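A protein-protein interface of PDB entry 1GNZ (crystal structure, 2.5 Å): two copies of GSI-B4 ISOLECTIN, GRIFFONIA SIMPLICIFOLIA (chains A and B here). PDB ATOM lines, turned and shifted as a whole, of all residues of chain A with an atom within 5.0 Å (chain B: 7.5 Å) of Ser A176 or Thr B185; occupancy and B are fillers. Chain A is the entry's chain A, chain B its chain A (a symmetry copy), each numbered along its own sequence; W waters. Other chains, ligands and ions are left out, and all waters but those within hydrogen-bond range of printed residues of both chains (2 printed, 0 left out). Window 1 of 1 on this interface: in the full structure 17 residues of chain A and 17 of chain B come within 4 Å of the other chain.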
ATOM      1  N   PHE A  71     -24.480  -9.572 -29.343  1.00  0.00           N
ATOM      2  CA  PHE A  71     -24.969  -8.606 -28.389  1.00  0.00           C
ATOM      3  C   PHE A  71     -23.902  -8.142 -27.431  1.00  0.00           C
ATOM      4  O   PHE A  71     -22.863  -8.790 -27.258  1.00  0.00           O
ATOM      5  CB  PHE A  71     -26.167  -9.154 -27.596  1.00  0.00           C
ATOM      6  CG  PHE A  71     -25.854 -10.365 -26.759  1.00  0.00           C
ATOM      7  CD1 PHE A  71     -26.132 -11.641 -27.228  1.00  0.00           C
ATOM      8  CD2 PHE A  71     -25.277 -10.227 -25.493  1.00  0.00           C
ATOM      9  CE1 PHE A  71     -25.851 -12.771 -26.447  1.00  0.00           C
ATOM     10  CE2 PHE A  71     -24.990 -11.341 -24.710  1.00  0.00           C
ATOM     11  CZ  PHE A  71     -25.277 -12.617 -25.186  1.00  0.00           C
ATOM     12  N   TYR A  72     -24.174  -6.992 -26.826  1.00  0.00           N
ATOM     13  CA  TYR A  72     -23.272  -6.394 -25.862  1.00  0.00           C
ATOM     14  C   TYR A  72     -24.092  -5.981 -24.655  1.00  0.00           C
ATOM     15  O   TYR A  72     -25.218  -5.508 -24.785  1.00  0.00           O
ATOM     16  CB  TYR A  72     -22.592  -5.161 -26.451  1.00  0.00           C
ATOM     17  CG  TYR A  72     -21.651  -4.508 -25.472  1.00  0.00           C
ATOM     18  CD1 TYR A  72     -20.450  -5.122 -25.109  1.00  0.00           C
ATOM     19  CD2 TYR A  72     -21.992  -3.302 -24.852  1.00  0.00           C
ATOM     20  CE1 TYR A  72     -19.616  -4.553 -24.153  1.00  0.00           C
ATOM     21  CE2 TYR A  72     -21.161  -2.724 -23.892  1.00  0.00           C
ATOM     22  CZ  TYR A  72     -19.980  -3.353 -23.547  1.00  0.00           C
ATOM     23  OH  TYR A  72     -19.164  -2.789 -22.593  1.00  0.00           O
ATOM     24  N   THR A  73     -23.548  -6.184 -23.470  1.00  0.00           N
ATOM     25  CA  THR A  73     -24.282  -5.774 -22.296  1.00  0.00           C
ATOM     26  C   THR A  73     -23.298  -5.214 -21.307  1.00  0.00           C
ATOM     27  O   THR A  73     -22.148  -5.659 -21.218  1.00  0.00           O
ATOM     28  CB  THR A  73     -25.068  -6.931 -21.633  1.00  0.00           C
ATOM     29  OG1 THR A  73     -26.035  -6.372 -20.736  1.00  0.00           O
ATOM     30  CG2 THR A  73     -24.134  -7.847 -20.831  1.00  0.00           C
ATOM     31  N   ARG A 174     -18.711  -6.164 -18.361  1.00  0.00           N
ATOM     32  CA  ARG A 174     -18.985  -6.051 -19.788  1.00  0.00           C
ATOM     33  C   ARG A 174     -19.029  -7.444 -20.409  1.00  0.00           C
ATOM     34  O   ARG A 174     -18.039  -8.189 -20.390  1.00  0.00           O
ATOM     35  CB  ARG A 174     -17.927  -5.198 -20.477  1.00  0.00           C
ATOM     36  CG  ARG A 174     -17.749  -3.836 -19.833  1.00  0.00           C
ATOM     37  CD  ARG A 174     -16.897  -2.943 -20.702  1.00  0.00           C
ATOM     38  NE  ARG A 174     -16.485  -1.716 -20.029  1.00  0.00           N
ATOM     39  CZ  ARG A 174     -15.667  -1.679 -18.981  1.00  0.00           C
ATOM     40  NH1 ARG A 174     -15.172  -2.808 -18.478  1.00  0.00           N
ATOM     41  NH2 ARG A 174     -15.319  -0.510 -18.456  1.00  0.00           N
ATOM     42  N   ILE A 175     -20.186  -7.791 -20.960  1.00  0.00           N
ATOM     43  CA  ILE A 175     -20.371  -9.093 -21.576  1.00  0.00           C
ATOM     44  C   ILE A 175     -20.750  -8.957 -23.048  1.00  0.00           C
ATOM     45  O   ILE A 175     -21.749  -8.324 -23.388  1.00  0.00           O
ATOM     46  CB  ILE A 175     -21.474  -9.872 -20.834  1.00  0.00           C
ATOM     47  CG1 ILE A 175     -21.094 -10.002 -19.358  1.00  0.00           C
ATOM     48  CG2 ILE A 175     -21.669 -11.250 -21.464  1.00  0.00           C
ATOM     49  CD1 ILE A 175     -22.202 -10.535 -18.487  1.00  0.00           C
ATOM     50  N   SER A 176     -19.945  -9.542 -23.926  1.00  0.00           N
ATOM     51  CA  SER A 176     -20.245  -9.478 -25.351  1.00  0.00           C
ATOM     52  C   SER A 176     -20.312 -10.869 -25.973  1.00  0.00           C
ATOM     53  O   SER A 176     -19.679 -11.826 -25.500  1.00  0.00           O
ATOM     54  CB  SER A 176     -19.211  -8.629 -26.097  1.00  0.00           C
ATOM     55  OG  SER A 176     -17.920  -9.194 -26.011  1.00  0.00           O
ATOM     56  N   TYR A 177     -21.105 -10.970 -27.030  1.00  0.00           N
ATOM     57  CA  TYR A 177     -21.270 -12.216 -27.734  1.00  0.00           C
ATOM     58  C   TYR A 177     -21.233 -12.008 -29.243  1.00  0.00           C
ATOM     59  O   TYR A 177     -22.040 -11.264 -29.799  1.00  0.00           O
ATOM     60  CB  TYR A 177     -22.594 -12.864 -27.357  1.00  0.00           C
ATOM     61  CG  TYR A 177     -22.767 -14.230 -27.984  1.00  0.00           C
ATOM     62  CD1 TYR A 177     -21.867 -15.262 -27.703  1.00  0.00           C
ATOM     63  CD2 TYR A 177     -23.806 -14.481 -28.881  1.00  0.00           C
ATOM     64  CE1 TYR A 177     -21.995 -16.506 -28.303  1.00  0.00           C
ATOM     65  CE2 TYR A 177     -23.947 -15.720 -29.487  1.00  0.00           C
ATOM     66  CZ  TYR A 177     -23.038 -16.732 -29.198  1.00  0.00           C
ATOM     67  OH  TYR A 177     -23.158 -17.961 -29.810  1.00  0.00           O
ATOM     68  N   ASP A 178     -20.284 -12.665 -29.899  1.00  0.00           N
ATOM     69  CA  ASP A 178     -20.152 -12.575 -31.346  1.00  0.00           C
ATOM     70  C   ASP A 178     -20.871 -13.811 -31.874  1.00  0.00           C
ATOM     71  O   ASP A 178     -20.338 -14.912 -31.834  1.00  0.00           O
ATOM     72  CB  ASP A 178     -18.665 -12.580 -31.737  1.00  0.00           C
ATOM     73  CG  ASP A 178     -18.442 -12.501 -33.240  1.00  0.00           C
ATOM     74  OD1 ASP A 178     -17.261 -12.454 -33.651  1.00  0.00           O
ATOM     75  OD2 ASP A 178     -19.431 -12.495 -34.013  1.00  0.00           O
ATOM     76  N   ILE A 183     -18.466 -16.578 -29.762  1.00  0.00           N
ATOM     77  CA  ILE A 183     -17.588 -16.365 -28.620  1.00  0.00           C
ATOM     78  C   ILE A 183     -18.236 -15.382 -27.651  1.00  0.00           C
ATOM     79  O   ILE A 183     -18.702 -14.312 -28.047  1.00  0.00           O
ATOM     80  CB  ILE A 183     -16.207 -15.809 -29.068  1.00  0.00           C
ATOM     81  CG1 ILE A 183     -15.494 -16.842 -29.958  1.00  0.00           C
ATOM     82  CG2 ILE A 183     -15.364 -15.462 -27.849  1.00  0.00           C
ATOM     83  CD1 ILE A 183     -14.108 -16.417 -30.435  1.00  0.00           C
ATOM     84  N   LEU A 184     -18.275 -15.772 -26.379  1.00  0.00           N
ATOM     85  CA  LEU A 184     -18.851 -14.954 -25.327  1.00  0.00           C
ATOM     86  C   LEU A 184     -17.670 -14.417 -24.520  1.00  0.00           C
ATOM     87  O   LEU A 184     -16.838 -15.195 -24.047  1.00  0.00           O
ATOM     88  CB  LEU A 184     -19.735 -15.816 -24.426  1.00  0.00           C
ATOM     89  CG  LEU A 184     -20.882 -15.155 -23.651  1.00  0.00           C
ATOM     90  CD1 LEU A 184     -21.345 -16.108 -22.583  1.00  0.00           C
ATOM     91  CD2 LEU A 184     -20.437 -13.871 -23.015  1.00  0.00           C
ATOM     92  N   THR A 185     -17.581 -13.097 -24.378  1.00  0.00           N
ATOM     93  CA  THR A 185     -16.487 -12.498 -23.609  1.00  0.00           C
ATOM     94  C   THR A 185     -17.023 -11.739 -22.414  1.00  0.00           C
ATOM     95  O   THR A 185     -18.082 -11.118 -22.490  1.00  0.00           O
ATOM     96  CB  THR A 185     -15.658 -11.478 -24.434  1.00  0.00           C
ATOM     97  OG1 THR A 185     -15.065 -12.124 -25.568  1.00  0.00           O
ATOM     98  CG2 THR A 185     -14.555 -10.872 -23.561  1.00  0.00           C
ATOM     99  N   SER A 199     -13.009 -15.324 -22.030  1.00  0.00           N
ATOM    100  CA  SER A 199     -13.677 -15.626 -23.296  1.00  0.00           C
ATOM    101  C   SER A 199     -13.753 -17.128 -23.530  1.00  0.00           C
ATOM    102  O   SER A 199     -12.832 -17.876 -23.177  1.00  0.00           O
ATOM    103  CB  SER A 199     -12.929 -14.993 -24.472  1.00  0.00           C
ATOM    104  OG  SER A 199     -12.846 -13.586 -24.366  1.00  0.00           O
ATOM    105  N   PHE B  71      -5.592  -8.222 -21.440  1.00  0.00           N
ATOM    106  CA  PHE B  71      -5.715  -6.786 -21.344  1.00  0.00           C
ATOM    107  C   PHE B  71      -7.029  -6.277 -21.876  1.00  0.00           C
ATOM    108  O   PHE B  71      -7.729  -6.962 -22.632  1.00  0.00           O
ATOM    109  CB  PHE B  71      -4.559  -6.074 -22.065  1.00  0.00           C
ATOM    110  CG  PHE B  71      -4.498  -6.334 -23.546  1.00  0.00           C
ATOM    111  CD1 PHE B  71      -3.648  -7.304 -24.059  1.00  0.00           C
ATOM    112  CD2 PHE B  71      -5.296  -5.605 -24.432  1.00  0.00           C
ATOM    113  CE1 PHE B  71      -3.581  -7.543 -25.440  1.00  0.00           C
ATOM    114  CE2 PHE B  71      -5.240  -5.835 -25.803  1.00  0.00           C
ATOM    115  CZ  PHE B  71      -4.381  -6.806 -26.311  1.00  0.00           C
ATOM    116  N   TYR B  72      -7.360  -5.064 -21.447  1.00  0.00           N
ATOM    117  CA  TYR B  72      -8.582  -4.405 -21.861  1.00  0.00           C
ATOM    118  C   TYR B  72      -8.227  -2.987 -22.266  1.00  0.00           C
ATOM    119  O   TYR B  72      -7.387  -2.341 -21.647  1.00  0.00           O
ATOM    120  CB  TYR B  72      -9.587  -4.361 -20.713  1.00  0.00           C
ATOM    121  CG  TYR B  72     -10.869  -3.674 -21.105  1.00  0.00           C
ATOM    122  CD1 TYR B  72     -11.762  -4.271 -21.999  1.00  0.00           C
ATOM    123  CD2 TYR B  72     -11.162  -2.390 -20.636  1.00  0.00           C
ATOM    124  CE1 TYR B  72     -12.910  -3.606 -22.415  1.00  0.00           C
ATOM    125  CE2 TYR B  72     -12.312  -1.715 -21.048  1.00  0.00           C
ATOM    126  CZ  TYR B  72     -13.176  -2.326 -21.935  1.00  0.00           C
ATOM    127  OH  TYR B  72     -14.306  -1.659 -22.351  1.00  0.00           O
ATOM    128  N   THR B  73      -8.844  -2.502 -23.328  1.00  0.00           N
ATOM    129  CA  THR B  73      -8.559  -1.144 -23.729  1.00  0.00           C
ATOM    130  C   THR B  73      -9.844  -0.523 -24.201  1.00  0.00           C
ATOM    131  O   THR B  73     -10.711  -1.190 -24.777  1.00  0.00           O
ATOM    132  CB  THR B  73      -7.504  -1.049 -24.856  1.00  0.00           C
ATOM    133  OG1 THR B  73      -7.021   0.299 -24.919  1.00  0.00           O
ATOM    134  CG2 THR B  73      -8.113  -1.411 -26.218  1.00  0.00           C
ATOM    135  N   VAL B 127      -6.273  -3.794 -34.475  1.00  0.00           N
ATOM    136  CA  VAL B 127      -7.707  -3.805 -34.712  1.00  0.00           C
ATOM    137  C   VAL B 127      -7.894  -2.533 -35.517  1.00  0.00           C
ATOM    138  O   VAL B 127      -7.629  -1.428 -35.030  1.00  0.00           O
ATOM    139  CB  VAL B 127      -8.520  -3.681 -33.405  1.00  0.00           C
ATOM    140  CG1 VAL B 127     -10.020  -3.710 -33.737  1.00  0.00           C
ATOM    141  CG2 VAL B 127      -8.143  -4.813 -32.439  1.00  0.00           C
ATOM    142  N   ILE B 147      -9.587  -7.437 -37.594  1.00  0.00           N
ATOM    143  CA  ILE B 147      -8.476  -7.805 -36.717  1.00  0.00           C
ATOM    144  C   ILE B 147      -7.308  -8.248 -37.598  1.00  0.00           C
ATOM    145  O   ILE B 147      -7.462  -9.130 -38.439  1.00  0.00           O
ATOM    146  CB  ILE B 147      -8.820  -8.976 -35.784  1.00  0.00           C
ATOM    147  CG1 ILE B 147      -9.990  -8.614 -34.876  1.00  0.00           C
ATOM    148  CG2 ILE B 147      -7.607  -9.310 -34.930  1.00  0.00           C
ATOM    149  CD1 ILE B 147     -10.383  -9.729 -33.904  1.00  0.00           C
ATOM    150  N   ARG B 174     -14.096  -0.891 -27.724  1.00  0.00           N
ATOM    151  CA  ARG B 174     -13.643  -1.708 -26.605  1.00  0.00           C
ATOM    152  C   ARG B 174     -12.929  -2.947 -27.136  1.00  0.00           C
ATOM    153  O   ARG B 174     -13.517  -3.776 -27.843  1.00  0.00           O
ATOM    154  CB  ARG B 174     -14.815  -2.112 -25.719  1.00  0.00           C
ATOM    155  CG  ARG B 174     -15.641  -0.929 -25.249  1.00  0.00           C
ATOM    156  CD  ARG B 174     -16.613  -1.351 -24.175  1.00  0.00           C
ATOM    157  NE  ARG B 174     -17.599  -0.323 -23.861  1.00  0.00           N
ATOM    158  CZ  ARG B 174     -18.532   0.097 -24.708  1.00  0.00           C
ATOM    159  NH1 ARG B 174     -18.609  -0.420 -25.932  1.00  0.00           N
ATOM    160  NH2 ARG B 174     -19.412   1.015 -24.321  1.00  0.00           N
ATOM    161  N   ILE B 175     -11.652  -3.068 -26.789  1.00  0.00           N
ATOM    162  CA  ILE B 175     -10.850  -4.193 -27.235  1.00  0.00           C
ATOM    163  C   ILE B 175     -10.304  -4.983 -26.049  1.00  0.00           C
ATOM    164  O   ILE B 175      -9.604  -4.441 -25.195  1.00  0.00           O
ATOM    165  CB  ILE B 175      -9.676  -3.690 -28.099  1.00  0.00           C
ATOM    166  CG1 ILE B 175     -10.225  -2.893 -29.282  1.00  0.00           C
ATOM    167  CG2 ILE B 175      -8.831  -4.866 -28.585  1.00  0.00           C
ATOM    168  CD1 ILE B 175      -9.171  -2.152 -30.062  1.00  0.00           C
ATOM    169  N   SER B 176     -10.633  -6.268 -25.990  1.00  0.00           N
ATOM    170  CA  SER B 176     -10.137  -7.101 -24.901  1.00  0.00           C
ATOM    171  C   SER B 176      -9.403  -8.331 -25.427  1.00  0.00           C
ATOM    172  O   SER B 176      -9.667  -8.825 -26.534  1.00  0.00           O
ATOM    173  CB  SER B 176     -11.276  -7.537 -23.975  1.00  0.00           C
ATOM    174  OG  SER B 176     -12.220  -8.336 -24.657  1.00  0.00           O
ATOM    175  N   TYR B 177      -8.463  -8.806 -24.621  1.00  0.00           N
ATOM    176  CA  TYR B 177      -7.686  -9.968 -24.970  1.00  0.00           C
ATOM    177  C   TYR B 177      -7.535 -10.910 -23.783  1.00  0.00           C
ATOM    178  O   TYR B 177      -7.016 -10.530 -22.735  1.00  0.00           O
ATOM    179  CB  TYR B 177      -6.302  -9.551 -25.449  1.00  0.00           C
ATOM    180  CG  TYR B 177      -5.482 -10.727 -25.934  1.00  0.00           C
ATOM    181  CD1 TYR B 177      -5.922 -11.506 -27.008  1.00  0.00           C
ATOM    182  CD2 TYR B 177      -4.290 -11.079 -25.301  1.00  0.00           C
ATOM    183  CE1 TYR B 177      -5.195 -12.609 -27.434  1.00  0.00           C
ATOM    184  CE2 TYR B 177      -3.554 -12.178 -25.718  1.00  0.00           C
ATOM    185  CZ  TYR B 177      -4.009 -12.944 -26.785  1.00  0.00           C
ATOM    186  OH  TYR B 177      -3.296 -14.048 -27.194  1.00  0.00           O
ATOM    187  N   ASP B 178      -8.004 -12.141 -23.953  1.00  0.00           N
ATOM    188  CA  ASP B 178      -7.902 -13.149 -22.908  1.00  0.00           C
ATOM    189  C   ASP B 178      -6.662 -13.957 -23.274  1.00  0.00           C
ATOM    190  O   ASP B 178      -6.701 -14.797 -24.163  1.00  0.00           O
ATOM    191  CB  ASP B 178      -9.164 -14.027 -22.903  1.00  0.00           C
ATOM    192  CG  ASP B 178      -9.130 -15.118 -21.843  1.00  0.00           C
ATOM    193  OD1 ASP B 178     -10.136 -15.855 -21.734  1.00  0.00           O
ATOM    194  OD2 ASP B 178      -8.109 -15.251 -21.126  1.00  0.00           O
ATOM    195  N   ILE B 183      -8.072 -15.098 -27.096  1.00  0.00           N
ATOM    196  CA  ILE B 183      -9.149 -14.533 -27.898  1.00  0.00           C
ATOM    197  C   ILE B 183      -9.138 -13.013 -27.772  1.00  0.00           C
ATOM    198  O   ILE B 183      -9.083 -12.467 -26.669  1.00  0.00           O
ATOM    199  CB  ILE B 183     -10.534 -15.076 -27.444  1.00  0.00           C
ATOM    200  CG1 ILE B 183     -10.597 -16.595 -27.671  1.00  0.00           C
ATOM    201  CG2 ILE B 183     -11.646 -14.362 -28.199  1.00  0.00           C
ATOM    202  CD1 ILE B 183     -11.927 -17.238 -27.289  1.00  0.00           C
ATOM    203  N   LEU B 184      -9.170 -12.342 -28.921  1.00  0.00           N
ATOM    204  CA  LEU B 184      -9.172 -10.892 -28.980  1.00  0.00           C
ATOM    205  C   LEU B 184     -10.592 -10.490 -29.376  1.00  0.00           C
ATOM    206  O   LEU B 184     -11.107 -10.959 -30.394  1.00  0.00           O
ATOM    207  CB  LEU B 184      -8.190 -10.416 -30.050  1.00  0.00           C
ATOM    208  CG  LEU B 184      -7.566  -9.020 -29.925  1.00  0.00           C
ATOM    209  CD1 LEU B 184      -6.954  -8.652 -31.249  1.00  0.00           C
ATOM    210  CD2 LEU B 184      -8.599  -7.997 -29.552  1.00  0.00           C
ATOM    211  N   THR B 185     -11.232  -9.645 -28.571  1.00  0.00           N
ATOM    212  CA  THR B 185     -12.592  -9.200 -28.883  1.00  0.00           C
ATOM    213  C   THR B 185     -12.631  -7.700 -29.089  1.00  0.00           C
ATOM    214  O   THR B 185     -11.920  -6.956 -28.416  1.00  0.00           O
ATOM    215  CB  THR B 185     -13.602  -9.506 -27.745  1.00  0.00           C
ATOM    216  OG1 THR B 185     -13.672 -10.919 -27.512  1.00  0.00           O
ATOM    217  CG2 THR B 185     -14.992  -8.986 -28.126  1.00  0.00           C
ATOM    218  N   VAL B 186     -13.481  -7.273 -30.016  1.00  0.00           N
ATOM    219  CA  VAL B 186     -13.669  -5.866 -30.313  1.00  0.00           C
ATOM    220  C   VAL B 186     -15.156  -5.542 -30.301  1.00  0.00           C
ATOM    221  O   VAL B 186     -15.955  -6.188 -30.990  1.00  0.00           O
ATOM    222  CB  VAL B 186     -13.115  -5.479 -31.717  1.00  0.00           C
ATOM    223  CG1 VAL B 186     -13.413  -4.009 -32.007  1.00  0.00           C
ATOM    224  CG2 VAL B 186     -11.622  -5.715 -31.772  1.00  0.00           C
ATOM    225  N   VAL B 187     -15.528  -4.559 -29.495  1.00  0.00           N
ATOM    226  CA  VAL B 187     -16.911  -4.116 -29.438  1.00  0.00           C
ATOM    227  C   VAL B 187     -16.881  -2.634 -29.815  1.00  0.00           C
ATOM    228  O   VAL B 187     -16.125  -1.857 -29.226  1.00  0.00           O
ATOM    229  CB  VAL B 187     -17.526  -4.260 -28.027  1.00  0.00           C
ATOM    230  CG1 VAL B 187     -19.003  -3.844 -28.067  1.00  0.00           C
ATOM    231  CG2 VAL B 187     -17.417  -5.690 -27.542  1.00  0.00           C
ATOM    232  N   TYR B 196     -21.175  -3.394 -32.526  1.00  0.00           N
ATOM    233  CA  TYR B 196     -20.480  -4.363 -33.350  1.00  0.00           C
ATOM    234  C   TYR B 196     -19.608  -5.238 -32.448  1.00  0.00           C
ATOM    235  O   TYR B 196     -18.790  -4.724 -31.675  1.00  0.00           O
ATOM    236  CB  TYR B 196     -19.576  -3.665 -34.374  1.00  0.00           C
ATOM    237  CG  TYR B 196     -20.273  -2.768 -35.379  1.00  0.00           C
ATOM    238  CD1 TYR B 196     -20.721  -1.489 -35.028  1.00  0.00           C
ATOM    239  CD2 TYR B 196     -20.477  -3.200 -36.690  1.00  0.00           C
ATOM    240  CE1 TYR B 196     -21.355  -0.667 -35.971  1.00  0.00           C
ATOM    241  CE2 TYR B 196     -21.102  -2.396 -37.629  1.00  0.00           C
ATOM    242  CZ  TYR B 196     -21.540  -1.135 -37.273  1.00  0.00           C
ATOM    243  OH  TYR B 196     -22.170  -0.362 -38.222  1.00  0.00           O
ATOM    244  N   ILE B 197     -19.790  -6.553 -32.526  1.00  0.00           N
ATOM    245  CA  ILE B 197     -18.966  -7.458 -31.735  1.00  0.00           C
ATOM    246  C   ILE B 197     -18.132  -8.333 -32.690  1.00  0.00           C
ATOM    247  O   ILE B 197     -18.673  -8.966 -33.591  1.00  0.00           O
ATOM    248  CB  ILE B 197     -19.821  -8.378 -30.815  1.00  0.00           C
ATOM    249  CG1 ILE B 197     -20.677  -7.546 -29.853  1.00  0.00           C
ATOM    250  CG2 ILE B 197     -18.914  -9.279 -30.003  1.00  0.00           C
ATOM    251  CD1 ILE B 197     -21.867  -6.860 -30.495  1.00  0.00           C
ATOM    252  N   LEU B 198     -16.817  -8.341 -32.512  1.00  0.00           N
ATOM    253  CA  LEU B 198     -15.930  -9.152 -33.354  1.00  0.00           C
ATOM    254  C   LEU B 198     -14.894  -9.853 -32.478  1.00  0.00           C
ATOM    255  O   LEU B 198     -14.164  -9.198 -31.729  1.00  0.00           O
ATOM    256  CB  LEU B 198     -15.214  -8.276 -34.388  1.00  0.00           C
ATOM    257  CG  LEU B 198     -14.219  -8.937 -35.358  1.00  0.00           C
ATOM    258  CD1 LEU B 198     -14.908 -10.029 -36.176  1.00  0.00           C
ATOM    259  CD2 LEU B 198     -13.644  -7.879 -36.278  1.00  0.00           C
ATOM    260  N   SER B 199     -14.846 -11.182 -32.566  1.00  0.00           N
ATOM    261  CA  SER B 199     -13.900 -11.972 -31.778  1.00  0.00           C
ATOM    262  C   SER B 199     -13.181 -12.993 -32.647  1.00  0.00           C
ATOM    263  O   SER B 199     -13.767 -13.563 -33.578  1.00  0.00           O
ATOM    264  CB  SER B 199     -14.619 -12.720 -30.652  1.00  0.00           C
ATOM    265  OG  SER B 199     -15.282 -11.846 -29.760  1.00  0.00           O
ATOM    266  N   HIS B 200     -11.912 -13.236 -32.325  1.00  0.00           N
ATOM    267  CA  HIS B 200     -11.120 -14.196 -33.069  1.00  0.00           C
ATOM    268  C   HIS B 200      -9.839 -14.545 -32.319  1.00  0.00           C
ATOM    269  O   HIS B 200      -9.381 -13.810 -31.443  1.00  0.00           O
ATOM    270  CB  HIS B 200     -10.805 -13.636 -34.458  1.00  0.00           C
ATOM    271  CG  HIS B 200     -10.334 -14.664 -35.439  1.00  0.00           C
ATOM    272  ND1 HIS B 200      -9.051 -15.188 -35.422  1.00  0.00           N
ATOM    273  CD2 HIS B 200     -10.973 -15.281 -36.458  1.00  0.00           C
ATOM    274  CE1 HIS B 200      -8.929 -16.073 -36.388  1.00  0.00           C
ATOM    275  NE2 HIS B 200     -10.081 -16.153 -37.037  1.00  0.00           N
ATOM    276  N   VAL B 202      -5.949 -15.103 -31.602  1.00  0.00           N
ATOM    277  CA  VAL B 202      -4.705 -14.413 -31.904  1.00  0.00           C
ATOM    278  C   VAL B 202      -3.647 -14.917 -30.937  1.00  0.00           C
ATOM    279  O   VAL B 202      -3.874 -14.968 -29.728  1.00  0.00           O
ATOM    280  CB  VAL B 202      -4.821 -12.879 -31.735  1.00  0.00           C
ATOM    281  CG1 VAL B 202      -3.470 -12.223 -32.012  1.00  0.00           C
ATOM    282  CG2 VAL B 202      -5.879 -12.328 -32.662  1.00  0.00           C
HETATM  283  O   HOH W   1     -17.100 -11.811 -27.495  1.00  0.00           O
HETATM  284  O   HOH W   2     -11.632 -11.251 -25.594  1.00  0.00           O
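Among the printed residues, pairs that only touch across the chains: Phe A71 with Ile B197, Tyr A72 with Val B187, Arg A174 with Arg B174, Ser A176 with Thr B185, Ser A176 with Val B187, Ser A176 with Ile B197, Tyr A177 with Ile B197, Asp A178 with Ile B197, Asp A178 with Leu B198, Ile A183 with Ile B183, Ile A183 with Ser B199, Thr A185 with Ser B176 and Ser A199 with Ile B183.
Of the printed residues of chain B, Phe A71 touches Ile B197 (3.6 Å). Ser A176 touches just these residues of chain B: Thr B185 (3.6 Å), Val B187 (3.7 Å) and Ile B197 (3.97 Å). Of the printed residues of chain B, Ile A183 touches Ile B183 (3.9 Å) and Ser B199 (3.7 Å). Of the printed residues of chain A, Thr B185 touches Ser A176 (3.6 Å) and Thr A185 (2.7 Å). Printed residues of chain A within 4 Å of Val B187: Tyr A72 and Ser A176. Printed residues of chain A within 4 Å of Ser B199: Asp A178 and Ile A183. The nearest residue of chain B that does not touch Ser A176 is Ser B199 (5.3 Å). The nearest printed residue of chain A that does not touch Leu B198 is Tyr A177 (6.6 Å).
Tyr A72 touches Arg B174, and with the chains exchanged Arg A174 touches Tyr B72. Ile B183 touches its own counterpart, Ile A183. Ile A183 touches Ser B199, and with the chains exchanged Ser A199 touches Ile B183. Thr A185 touches its own counterpart, Thr B185. Of the 18 pairs that touch across the chains among the printed residues, 11 have their exchanged pair printed and touching as well.
Of the 12 printed residues of chain A, 9 touch a printed residue of chain B. Hydrophobic or aromatic side chains of chain A within 4 Å of the printed part of chain B: Tyr A72 and Ile A183. Of the 21 printed residues of chain B, 10 touch a printed residue of chain A. Among the printed residues, 18 pairs touch across the chains. Among the printed residues, no Asp or Glu carboxylate lies within 4 Å of a Lys or Arg side-chain nitrogen of the other chain.
The guanidinium group (NE) of Arg B174 sits at hydrogen-bond distance from the side-chain hydroxyl (OH) of Tyr A72 (3.2 Å). The guanidinium group of Arg A174 lies within hydrogen-bond range of the side-chain hydroxyl of Tyr B72 (3.2 Å). The side-chain carboxylate of Asp A178 is in hydrogen-bond range of the backbone NH of Ser B199 (2.9 Å). The side-chain hydroxyl of Thr B185 sits at hydrogen-bond distance from the side-chain hydroxyl of Thr A185. The backbone NH of Ser A199 lies within hydrogen-bond range of the side-chain carboxylate of Asp B178.
Water W2 lies within hydrogen-bond range of the side-chain hydroxyl (OG1) of Thr B185 (2.8 Å), the side-chain hydroxyl (OG) of Ser A199 (2.9 Å), the backbone carbonyl oxygen (O) of Ile B183 (3.0 Å) and the side-chain hydroxyl (OG) of Ser B176 (3.1 Å). Water W1 lies within hydrogen-bond range of the side-chain hydroxyl (OG1) of Thr A185 (2.8 Å), the side-chain hydroxyl (OG) of Ser B199 (2.9 Å), the backbone carbonyl oxygen (O) of Ile A183 (3.0 Å) and the side-chain hydroxyl (OG) of Ser A176 (3.1 Å).
O of Phe A71 lies within hydrogen-bond range of N of Tyr A177, at 2.8 Å. The backbone NH (N) of Thr A185 lies within hydrogen-bond range of the backbone carbonyl oxygen (O) of Ser A176, 2.7 Å away. OG1 of Thr A185 is in hydrogen-bond range of OG of Ser A199, 2.9 Å away. The backbone NH (N) of Arg B174 lies within hydrogen-bond range of the backbone carbonyl oxygen (O) of Val B187 (2.7 Å). N of Asp B178 sits at hydrogen-bond distance from O of Ile B183 (2.9 Å). The backbone carbonyl oxygen of Leu B198 lies within hydrogen-bond range of the backbone NH of Val B186, 2.7 Å away.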
